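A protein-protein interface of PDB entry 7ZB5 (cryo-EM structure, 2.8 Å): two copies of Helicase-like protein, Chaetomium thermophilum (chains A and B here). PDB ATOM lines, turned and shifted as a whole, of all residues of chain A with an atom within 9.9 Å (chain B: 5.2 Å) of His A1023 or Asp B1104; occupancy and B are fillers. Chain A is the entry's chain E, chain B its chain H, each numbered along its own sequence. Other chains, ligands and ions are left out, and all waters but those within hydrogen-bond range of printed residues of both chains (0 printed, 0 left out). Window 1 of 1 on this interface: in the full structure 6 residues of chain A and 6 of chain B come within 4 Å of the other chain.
OD1 of Asp A1104 sits close to N of Glu A1106. NE2 of His A1023 sits at hydrogen-bond distance from O of Pro A1019, 3.1 Å away. N of Glu B1106 lies close to OD1 of Asp B1104, at 3.4 Å.
His A1023 touches four residues of chain B. Asp B1104 touches just one residue of chain A: His A1023 (3.5 Å). Printed residues of chain A within 4 Å of Pro B1105: His A1023 (3.2 Å). Glu B1106 touches one residue of chain A. Asn B1107 touches none of the printed residues of chain A. Printed residues of chain B within 4 Å of Pro A1105: His B1023 (3.4 Å). Of the printed residues of chain B, Glu A1106 touches His B1023. Of the printed residues of chain A, His B1023 touches His A1023 (3.9 Å), Asp A1104 (3.5 Å), Pro A1105 (3.4 Å) and Glu A1106 (3.5 Å). Printed residues of chain A within 4 Å of Arg B1103: Pro A1100. Ala B1022 touches none of the printed residues of chain A. The nearest printed residue of chain B that does not touch His A1023 is Asn B1107 (6.0 Å). The nearest residue of chain A that does not touch Asp B1104 is Ala A1022 (4.02 Å). The nearest printed residue of chain A that does not touch Arg B1103 is Arg A1103 (4.4 Å).
Among the printed residues, pairs that only touch across the chains: His A1023 with Pro B1105 (3.2 Å), His A1023 with Glu B1106 (3.3 Å), Pro A1105 with His B1023 (3.4 Å), His A1023 with Asp B1104 (3.5 Å), Asp A1104 with His B1023 (3.5 Å), Glu A1106 with His B1023 (3.5 Å), Pro A1100 with Arg B1103 (3.5 Å), Arg A1103 with Pro B1100 (3.6 Å) and His A1023 with His B1023 (3.9 Å).
His B1023 touches its own counterpart, His A1023. His A1023 touches Asp B1104, and with the chains exchanged Asp A1104 touches His B1023. His A1023 touches Glu B1106, and with the chains exchanged Glu A1106 touches His B1023. Pro A1100 touches Arg B1103, and with the chains exchanged Arg A1103 touches Pro B1100. 9 positions are printed for both chains. Of the 9 pairs that touch across the chains among the printed residues, 9 have their exchanged pair printed and touching as well.
Hydrophobic or aromatic side chains of chain A that line the printed part of chain B: His A1023, Pro A1100 and Pro A1105. Among the printed residues, no Asp or Glu carboxylate lies within 4 Å of a Lys or Arg side-chain nitrogen of the other chain.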
ATOM      1  N   GLU A1017       4.293   7.067  11.915  1.00  0.00           N
ATOM      2  CA  GLU A1017       4.757   6.053  10.977  1.00  0.00           C
ATOM      3  C   GLU A1017       3.556   5.251  10.487  1.00  0.00           C
ATOM      4  O   GLU A1017       2.915   4.535  11.265  1.00  0.00           O
ATOM      5  CB  GLU A1017       5.801   5.153  11.628  1.00  0.00           C
ATOM      6  CG  GLU A1017       7.159   5.814  11.784  1.00  0.00           C
ATOM      7  CD  GLU A1017       8.242   4.834  12.189  1.00  0.00           C
ATOM      8  OE1 GLU A1017       7.911   3.667  12.485  1.00  0.00           O
ATOM      9  OE2 GLU A1017       9.425   5.232  12.208  1.00  0.00           O
ATOM     10  N   PHE A1018       3.248   5.384   9.199  1.00  0.00           N
ATOM     11  CA  PHE A1018       2.125   4.667   8.599  1.00  0.00           C
ATOM     12  C   PHE A1018       2.169   3.153   8.780  1.00  0.00           C
ATOM     13  O   PHE A1018       1.102   2.566   9.028  1.00  0.00           O
ATOM     14  CB  PHE A1018       2.049   5.011   7.105  1.00  0.00           C
ATOM     15  CG  PHE A1018       1.379   3.958   6.277  1.00  0.00           C
ATOM     16  CD1 PHE A1018       0.001   3.844   6.261  1.00  0.00           C
ATOM     17  CD2 PHE A1018       2.129   3.086   5.510  1.00  0.00           C
ATOM     18  CE1 PHE A1018      -0.618   2.877   5.497  1.00  0.00           C
ATOM     19  CE2 PHE A1018       1.519   2.120   4.747  1.00  0.00           C
ATOM     20  CZ  PHE A1018       0.142   2.012   4.739  1.00  0.00           C
ATOM     21  N   PRO A1019       3.311   2.466   8.648  1.00  0.00           N
ATOM     22  CA  PRO A1019       3.305   0.999   8.815  1.00  0.00           C
ATOM     23  C   PRO A1019       2.745   0.513  10.144  1.00  0.00           C
ATOM     24  O   PRO A1019       2.345  -0.655  10.234  1.00  0.00           O
ATOM     25  CB  PRO A1019       4.786   0.629   8.674  1.00  0.00           C
ATOM     26  CG  PRO A1019       5.344   1.677   7.798  1.00  0.00           C
ATOM     27  CD  PRO A1019       4.602   2.939   8.117  1.00  0.00           C
ATOM     28  N   ILE A1020       2.697   1.359  11.169  1.00  0.00           N
ATOM     29  CA  ILE A1020       2.135   0.968  12.457  1.00  0.00           C
ATOM     30  C   ILE A1020       0.623   1.153  12.479  1.00  0.00           C
ATOM     31  O   ILE A1020      -0.103   0.290  12.979  1.00  0.00           O
ATOM     32  CB  ILE A1020       2.814   1.769  13.588  1.00  0.00           C
ATOM     33  CG1 ILE A1020       4.345   1.701  13.477  1.00  0.00           C
ATOM     34  CG2 ILE A1020       2.343   1.269  14.954  1.00  0.00           C
ATOM     35  CD1 ILE A1020       4.920   0.299  13.384  1.00  0.00           C
ATOM     36  N   HIS A1021       0.130   2.263  11.935  1.00  0.00           N
ATOM     37  CA  HIS A1021      -1.284   2.611  11.988  1.00  0.00           C
ATOM     38  C   HIS A1021      -2.051   2.169  10.748  1.00  0.00           C
ATOM     39  O   HIS A1021      -3.221   2.532  10.596  1.00  0.00           O
ATOM     40  CB  HIS A1021      -1.441   4.120  12.186  1.00  0.00           C
ATOM     41  CG  HIS A1021      -0.809   4.628  13.442  1.00  0.00           C
ATOM     42  ND1 HIS A1021      -1.454   4.610  14.659  1.00  0.00           N
ATOM     43  CD2 HIS A1021       0.413   5.164  13.672  1.00  0.00           C
ATOM     44  CE1 HIS A1021      -0.658   5.113  15.585  1.00  0.00           C
ATOM     45  NE2 HIS A1021       0.481   5.458  15.012  1.00  0.00           N
ATOM     46  N   ALA A1022      -1.421   1.406   9.854  1.00  0.00           N
ATOM     47  CA  ALA A1022      -2.126   0.895   8.687  1.00  0.00           C
ATOM     48  C   ALA A1022      -3.229  -0.088   9.059  1.00  0.00           C
ATOM     49  O   ALA A1022      -4.152  -0.296   8.263  1.00  0.00           O
ATOM     50  CB  ALA A1022      -1.138   0.223   7.734  1.00  0.00           C
ATOM     51  N   HIS A1023      -3.159  -0.691  10.247  1.00  0.00           N
ATOM     52  CA  HIS A1023      -4.082  -1.742  10.655  1.00  0.00           C
ATOM     53  C   HIS A1023      -5.209  -1.230  11.545  1.00  0.00           C
ATOM     54  O   HIS A1023      -6.003  -2.038  12.037  1.00  0.00           O
ATOM     55  CB  HIS A1023      -3.328  -2.858  11.380  1.00  0.00           C
ATOM     56  CG  HIS A1023      -1.890  -2.981  10.982  1.00  0.00           C
ATOM     57  ND1 HIS A1023      -1.484  -3.667   9.859  1.00  0.00           N
ATOM     58  CD2 HIS A1023      -0.763  -2.502  11.560  1.00  0.00           C
ATOM     59  CE1 HIS A1023      -0.167  -3.607   9.762  1.00  0.00           C
ATOM     60  NE2 HIS A1023       0.294  -2.906  10.781  1.00  0.00           N
ATOM     61  N   LYS A1024      -5.303   0.081  11.761  1.00  0.00           N
ATOM     62  CA  LYS A1024      -6.296   0.675  12.646  1.00  0.00           C
ATOM     63  C   LYS A1024      -7.355   1.390  11.822  1.00  0.00           C
ATOM     64  O   LYS A1024      -7.028   2.189  10.940  1.00  0.00           O
ATOM     65  CB  LYS A1024      -5.638   1.646  13.628  1.00  0.00           C
ATOM     66  CG  LYS A1024      -5.600   1.122  15.054  1.00  0.00           C
ATOM     67  CD  LYS A1024      -4.720   1.968  15.955  1.00  0.00           C
ATOM     68  CE  LYS A1024      -3.251   1.633  15.776  1.00  0.00           C
ATOM     69  NZ  LYS A1024      -2.396   2.323  16.777  1.00  0.00           N
ATOM     70  N   THR A1025      -8.621   1.094  12.112  1.00  0.00           N
ATOM     71  CA  THR A1025      -9.753   1.672  11.403  1.00  0.00           C
ATOM     72  C   THR A1025     -10.821   2.074  12.407  1.00  0.00           C
ATOM     73  O   THR A1025     -11.080   1.351  13.374  1.00  0.00           O
ATOM     74  CB  THR A1025     -10.338   0.685  10.385  1.00  0.00           C
ATOM     75  OG1 THR A1025      -9.317   0.284   9.461  1.00  0.00           O
ATOM     76  CG2 THR A1025     -11.491   1.318   9.617  1.00  0.00           C
ATOM     77  N   ASN A1026     -11.443   3.230  12.164  1.00  0.00           N
ATOM     78  CA  ASN A1026     -12.526   3.743  13.005  1.00  0.00           C
ATOM     79  C   ASN A1026     -12.092   3.878  14.463  1.00  0.00           C
ATOM     80  O   ASN A1026     -12.826   3.512  15.383  1.00  0.00           O
ATOM     81  CB  ASN A1026     -13.771   2.865  12.893  1.00  0.00           C
ATOM     82  CG  ASN A1026     -14.329   2.829  11.488  1.00  0.00           C
ATOM     83  OD1 ASN A1026     -14.043   3.706  10.674  1.00  0.00           O
ATOM     84  ND2 ASN A1026     -15.134   1.815  11.196  1.00  0.00           N
ATOM     85  N   VAL A1027     -10.885   4.399  14.672  1.00  0.00           N
ATOM     86  CA  VAL A1027     -10.382   4.738  15.997  1.00  0.00           C
ATOM     87  C   VAL A1027      -9.906   6.181  15.961  1.00  0.00           C
ATOM     88  O   VAL A1027      -9.308   6.621  14.974  1.00  0.00           O
ATOM     89  CB  VAL A1027      -9.242   3.800  16.449  1.00  0.00           C
ATOM     90  CG1 VAL A1027      -9.678   2.347  16.333  1.00  0.00           C
ATOM     91  CG2 VAL A1027      -7.973   4.059  15.647  1.00  0.00           C
ATOM     92  N   LEU A1029      -7.370   8.624  16.631  1.00  0.00           N
ATOM     93  CA  LEU A1029      -5.939   8.598  16.916  1.00  0.00           C
ATOM     94  C   LEU A1029      -5.575   9.547  18.049  1.00  0.00           C
ATOM     95  O   LEU A1029      -4.608   9.301  18.778  1.00  0.00           O
ATOM     96  CB  LEU A1029      -5.146   8.957  15.658  1.00  0.00           C
ATOM     97  CG  LEU A1029      -4.978   7.876  14.586  1.00  0.00           C
ATOM     98  CD1 LEU A1029      -6.307   7.507  13.942  1.00  0.00           C
ATOM     99  CD2 LEU A1029      -3.984   8.335  13.530  1.00  0.00           C
ATOM    100  N   PRO A1100      -5.343   0.314  -4.106  1.00  0.00           N
ATOM    101  CA  PRO A1100      -5.278  -0.727  -3.070  1.00  0.00           C
ATOM    102  C   PRO A1100      -3.976  -0.711  -2.290  1.00  0.00           C
ATOM    103  O   PRO A1100      -3.963  -1.082  -1.111  1.00  0.00           O
ATOM    104  CB  PRO A1100      -5.449  -2.029  -3.865  1.00  0.00           C
ATOM    105  CG  PRO A1100      -6.178  -1.629  -5.086  1.00  0.00           C
ATOM    106  CD  PRO A1100      -5.665  -0.265  -5.425  1.00  0.00           C
ATOM    107  N   ALA A1102      -2.538   1.839  -1.217  1.00  0.00           N
ATOM    108  CA  ALA A1102      -2.610   2.865  -0.184  1.00  0.00           C
ATOM    109  C   ALA A1102      -2.825   2.254   1.193  1.00  0.00           C
ATOM    110  O   ALA A1102      -2.424   2.844   2.203  1.00  0.00           O
ATOM    111  CB  ALA A1102      -3.731   3.854  -0.503  1.00  0.00           C
ATOM    112  N   ARG A1103      -3.447   1.078   1.253  1.00  0.00           N
ATOM    113  CA  ARG A1103      -3.659   0.350   2.495  1.00  0.00           C
ATOM    114  C   ARG A1103      -2.571  -0.685   2.762  1.00  0.00           C
ATOM    115  O   ARG A1103      -2.677  -1.440   3.732  1.00  0.00           O
ATOM    116  CB  ARG A1103      -5.027  -0.334   2.470  1.00  0.00           C
ATOM    117  CG  ARG A1103      -6.202   0.623   2.368  1.00  0.00           C
ATOM    118  CD  ARG A1103      -7.482  -0.109   2.026  1.00  0.00           C
ATOM    119  NE  ARG A1103      -8.599   0.809   1.828  1.00  0.00           N
ATOM    120  CZ  ARG A1103      -9.411   1.247   2.783  1.00  0.00           C
ATOM    121  NH1 ARG A1103      -9.264   0.885   4.048  1.00  0.00           N
ATOM    122  NH2 ARG A1103     -10.403   2.072   2.460  1.00  0.00           N
ATOM    123  N   ASP A1104      -1.530  -0.736   1.931  1.00  0.00           N
ATOM    124  CA  ASP A1104      -0.488  -1.743   2.073  1.00  0.00           C
ATOM    125  C   ASP A1104       0.581  -1.235   3.034  1.00  0.00           C
ATOM    126  O   ASP A1104       1.160  -0.171   2.779  1.00  0.00           O
ATOM    127  CB  ASP A1104       0.137  -2.055   0.725  1.00  0.00           C
ATOM    128  CG  ASP A1104       1.100  -3.227   0.783  1.00  0.00           C
ATOM    129  OD1 ASP A1104       1.165  -3.900   1.834  1.00  0.00           O
ATOM    130  OD2 ASP A1104       1.794  -3.476  -0.226  1.00  0.00           O
ATOM    131  N   PRO A1105       0.871  -1.931   4.141  1.00  0.00           N
ATOM    132  CA  PRO A1105       1.945  -1.452   5.026  1.00  0.00           C
ATOM    133  C   PRO A1105       3.314  -1.377   4.369  1.00  0.00           C
ATOM    134  O   PRO A1105       4.122  -0.523   4.754  1.00  0.00           O
ATOM    135  CB  PRO A1105       1.919  -2.467   6.175  1.00  0.00           C
ATOM    136  CG  PRO A1105       0.504  -2.880   6.234  1.00  0.00           C
ATOM    137  CD  PRO A1105       0.109  -3.012   4.793  1.00  0.00           C
ATOM    138  N   GLU A1106       3.602  -2.231   3.388  1.00  0.00           N
ATOM    139  CA  GLU A1106       4.915  -2.264   2.753  1.00  0.00           C
ATOM    140  C   GLU A1106       5.034  -1.327   1.556  1.00  0.00           C
ATOM    141  O   GLU A1106       6.120  -1.231   0.976  1.00  0.00           O
ATOM    142  CB  GLU A1106       5.252  -3.694   2.318  1.00  0.00           C
ATOM    143  CG  GLU A1106       5.868  -4.553   3.416  1.00  0.00           C
ATOM    144  CD  GLU A1106       7.284  -4.141   3.771  1.00  0.00           C
ATOM    145  OE1 GLU A1106       7.823  -3.223   3.118  1.00  0.00           O
ATOM    146  OE2 GLU A1106       7.860  -4.737   4.706  1.00  0.00           O
ATOM    147  N   LEU A1150     -10.316   6.897   5.522  1.00  0.00           N
ATOM    148  CA  LEU A1150      -8.979   6.608   6.023  1.00  0.00           C
ATOM    149  C   LEU A1150      -8.752   7.402   7.305  1.00  0.00           C
ATOM    150  O   LEU A1150      -8.929   8.625   7.321  1.00  0.00           O
ATOM    151  CB  LEU A1150      -7.929   6.950   4.969  1.00  0.00           C
ATOM    152  CG  LEU A1150      -7.677   5.958   3.826  1.00  0.00           C
ATOM    153  CD1 LEU A1150      -7.169   4.618   4.342  1.00  0.00           C
ATOM    154  CD2 LEU A1150      -8.928   5.769   2.974  1.00  0.00           C
ATOM    155  N   SER A1151      -8.378   6.707   8.382  1.00  0.00           N
ATOM    156  CA  SER A1151      -8.264   7.360   9.683  1.00  0.00           C
ATOM    157  C   SER A1151      -7.173   8.424   9.681  1.00  0.00           C
ATOM    158  O   SER A1151      -7.368   9.522  10.215  1.00  0.00           O
ATOM    159  CB  SER A1151      -7.991   6.319  10.767  1.00  0.00           C
ATOM    160  OG  SER A1151      -6.755   5.667  10.547  1.00  0.00           O
ATOM    161  N   VAL A1152      -6.015   8.119   9.091  1.00  0.00           N
ATOM    162  CA  VAL A1152      -4.934   9.100   9.054  1.00  0.00           C
ATOM    163  C   VAL A1152      -5.309  10.274   8.168  1.00  0.00           C
ATOM    164  O   VAL A1152      -4.894  11.410   8.431  1.00  0.00           O
ATOM    165  CB  VAL A1152      -3.613   8.458   8.594  1.00  0.00           C
ATOM    166  CG1 VAL A1152      -3.199   7.341   9.547  1.00  0.00           C
ATOM    167  CG2 VAL A1152      -3.714   7.965   7.149  1.00  0.00           C
ATOM    168  N   PHE B1018      -2.124 -15.218   7.334  1.00  0.00           N
ATOM    169  CA  PHE B1018      -2.353 -14.007   6.549  1.00  0.00           C
ATOM    170  C   PHE B1018      -1.706 -12.753   7.125  1.00  0.00           C
ATOM    171  O   PHE B1018      -1.169 -11.959   6.335  1.00  0.00           O
ATOM    172  CB  PHE B1018      -3.864 -13.788   6.386  1.00  0.00           C
ATOM    173  CG  PHE B1018      -4.240 -12.367   6.095  1.00  0.00           C
ATOM    174  CD1 PHE B1018      -4.116 -11.852   4.816  1.00  0.00           C
ATOM    175  CD2 PHE B1018      -4.729 -11.547   7.098  1.00  0.00           C
ATOM    176  CE1 PHE B1018      -4.464 -10.546   4.544  1.00  0.00           C
ATOM    177  CE2 PHE B1018      -5.076 -10.242   6.832  1.00  0.00           C
ATOM    178  CZ  PHE B1018      -4.945  -9.739   5.554  1.00  0.00           C
ATOM    179  N   ALA B1022       0.096 -10.504   4.395  1.00  0.00           N
ATOM    180  CA  ALA B1022      -0.785  -9.442   3.930  1.00  0.00           C
ATOM    181  C   ALA B1022      -0.026  -8.337   3.208  1.00  0.00           C
ATOM    182  O   ALA B1022      -0.617  -7.630   2.384  1.00  0.00           O
ATOM    183  CB  ALA B1022      -1.558  -8.850   5.109  1.00  0.00           C
ATOM    184  N   HIS B1023       1.264  -8.172   3.495  1.00  0.00           N
ATOM    185  CA  HIS B1023       2.057  -7.076   2.959  1.00  0.00           C
ATOM    186  C   HIS B1023       2.804  -7.447   1.684  1.00  0.00           C
ATOM    187  O   HIS B1023       3.590  -6.632   1.188  1.00  0.00           O
ATOM    188  CB  HIS B1023       3.068  -6.593   4.004  1.00  0.00           C
ATOM    189  CG  HIS B1023       2.516  -6.481   5.392  1.00  0.00           C
ATOM    190  ND1 HIS B1023       3.295  -6.665   6.514  1.00  0.00           N
ATOM    191  CD2 HIS B1023       1.273  -6.193   5.842  1.00  0.00           C
ATOM    192  CE1 HIS B1023       2.554  -6.503   7.595  1.00  0.00           C
ATOM    193  NE2 HIS B1023       1.323  -6.216   7.216  1.00  0.00           N
ATOM    194  N   PRO B1100     -12.370  -3.631   1.287  1.00  0.00           N
ATOM    195  CA  PRO B1100     -11.069  -3.068   1.681  1.00  0.00           C
ATOM    196  C   PRO B1100     -10.457  -3.770   2.879  1.00  0.00           C
ATOM    197  O   PRO B1100      -9.227  -3.835   2.988  1.00  0.00           O
ATOM    198  CB  PRO B1100     -11.395  -1.601   1.987  1.00  0.00           C
ATOM    199  CG  PRO B1100     -12.618  -1.315   1.208  1.00  0.00           C
ATOM    200  CD  PRO B1100     -13.409  -2.585   1.231  1.00  0.00           C
ATOM    201  N   GLU B1101     -11.283  -4.300   3.784  1.00  0.00           N
ATOM    202  CA  GLU B1101     -10.769  -5.022   4.942  1.00  0.00           C
ATOM    203  C   GLU B1101     -10.163  -6.371   4.574  1.00  0.00           C
ATOM    204  O   GLU B1101      -9.492  -6.976   5.417  1.00  0.00           O
ATOM    205  CB  GLU B1101     -11.875  -5.218   5.986  1.00  0.00           C
ATOM    206  CG  GLU B1101     -13.136  -5.934   5.491  1.00  0.00           C
ATOM    207  CD  GLU B1101     -14.231  -4.977   5.050  1.00  0.00           C
ATOM    208  OE1 GLU B1101     -13.908  -3.833   4.665  1.00  0.00           O
ATOM    209  OE2 GLU B1101     -15.415  -5.371   5.088  1.00  0.00           O
ATOM    210  N   ALA B1102     -10.377  -6.854   3.347  1.00  0.00           N
ATOM    211  CA  ALA B1102      -9.697  -8.062   2.900  1.00  0.00           C
ATOM    212  C   ALA B1102      -8.189  -7.878   2.852  1.00  0.00           C
ATOM    213  O   ALA B1102      -7.451  -8.864   2.964  1.00  0.00           O
ATOM    214  CB  ALA B1102     -10.213  -8.477   1.522  1.00  0.00           C
ATOM    215  N   ARG B1103      -7.718  -6.642   2.692  1.00  0.00           N
ATOM    216  CA  ARG B1103      -6.300  -6.318   2.692  1.00  0.00           C
ATOM    217  C   ARG B1103      -5.816  -5.807   4.044  1.00  0.00           C
ATOM    218  O   ARG B1103      -4.671  -5.355   4.148  1.00  0.00           O
ATOM    219  CB  ARG B1103      -6.005  -5.277   1.610  1.00  0.00           C
ATOM    220  CG  ARG B1103      -6.327  -5.734   0.198  1.00  0.00           C
ATOM    221  CD  ARG B1103      -6.304  -4.571  -0.772  1.00  0.00           C
ATOM    222  NE  ARG B1103      -6.684  -4.979  -2.121  1.00  0.00           N
ATOM    223  CZ  ARG B1103      -5.855  -5.456  -3.040  1.00  0.00           C
ATOM    224  NH1 ARG B1103      -4.563  -5.622  -2.798  1.00  0.00           N
ATOM    225  NH2 ARG B1103      -6.333  -5.780  -4.237  1.00  0.00           N
ATOM    226  N   ASP B1104      -6.654  -5.868   5.078  1.00  0.00           N
ATOM    227  CA  ASP B1104      -6.298  -5.332   6.383  1.00  0.00           C
ATOM    228  C   ASP B1104      -5.617  -6.420   7.205  1.00  0.00           C
ATOM    229  O   ASP B1104      -6.225  -7.476   7.424  1.00  0.00           O
ATOM    230  CB  ASP B1104      -7.534  -4.835   7.109  1.00  0.00           C
ATOM    231  CG  ASP B1104      -7.203  -4.105   8.399  1.00  0.00           C
ATOM    232  OD1 ASP B1104      -6.008  -3.842   8.651  1.00  0.00           O
ATOM    233  OD2 ASP B1104      -8.142  -3.793   9.162  1.00  0.00           O
ATOM    234  N   PRO B1105      -4.373  -6.231   7.666  1.00  0.00           N
ATOM    235  CA  PRO B1105      -3.751  -7.280   8.492  1.00  0.00           C
ATOM    236  C   PRO B1105      -4.490  -7.581   9.786  1.00  0.00           C
ATOM    237  O   PRO B1105      -4.443  -8.725  10.255  1.00  0.00           O
ATOM    238  CB  PRO B1105      -2.347  -6.721   8.756  1.00  0.00           C
ATOM    239  CG  PRO B1105      -2.077  -5.874   7.577  1.00  0.00           C
ATOM    240  CD  PRO B1105      -3.383  -5.202   7.296  1.00  0.00           C
ATOM    241  N   GLU B1106      -5.176  -6.602  10.376  1.00  0.00           N
ATOM    242  CA  GLU B1106      -5.856  -6.792  11.651  1.00  0.00           C
ATOM    243  C   GLU B1106      -7.294  -7.279  11.505  1.00  0.00           C
ATOM    244  O   GLU B1106      -7.959  -7.496  12.523  1.00  0.00           O
ATOM    245  CB  GLU B1106      -5.837  -5.488  12.457  1.00  0.00           C
ATOM    246  CG  GLU B1106      -4.581  -5.290  13.300  1.00  0.00           C
ATOM    247  CD  GLU B1106      -4.512  -6.227  14.493  1.00  0.00           C
ATOM    248  OE1 GLU B1106      -5.468  -7.002  14.701  1.00  0.00           O
ATOM    249  OE2 GLU B1106      -3.498  -6.187  15.221  1.00  0.00           O
ATOM    250  N   ASN B1107      -7.786  -7.463  10.283  1.00  0.00           N
ATOM    251  CA  ASN B1107      -9.112  -8.019  10.058  1.00  0.00           C
ATOM    252  C   ASN B1107      -9.010  -9.536   9.962  1.00  0.00           C
ATOM    253  O   ASN B1107      -8.213 -10.064   9.179  1.00  0.00           O
ATOM    254  CB  ASN B1107      -9.729  -7.447   8.783  1.00  0.00           C
ATOM    255  CG  ASN B1107     -11.200  -7.767   8.656  1.00  0.00           C
ATOM    256  OD1 ASN B1107     -11.582  -8.767   8.052  1.00  0.00           O
ATOM    257  ND2 ASN B1107     -12.039  -6.914   9.231  1.00  0.00           N
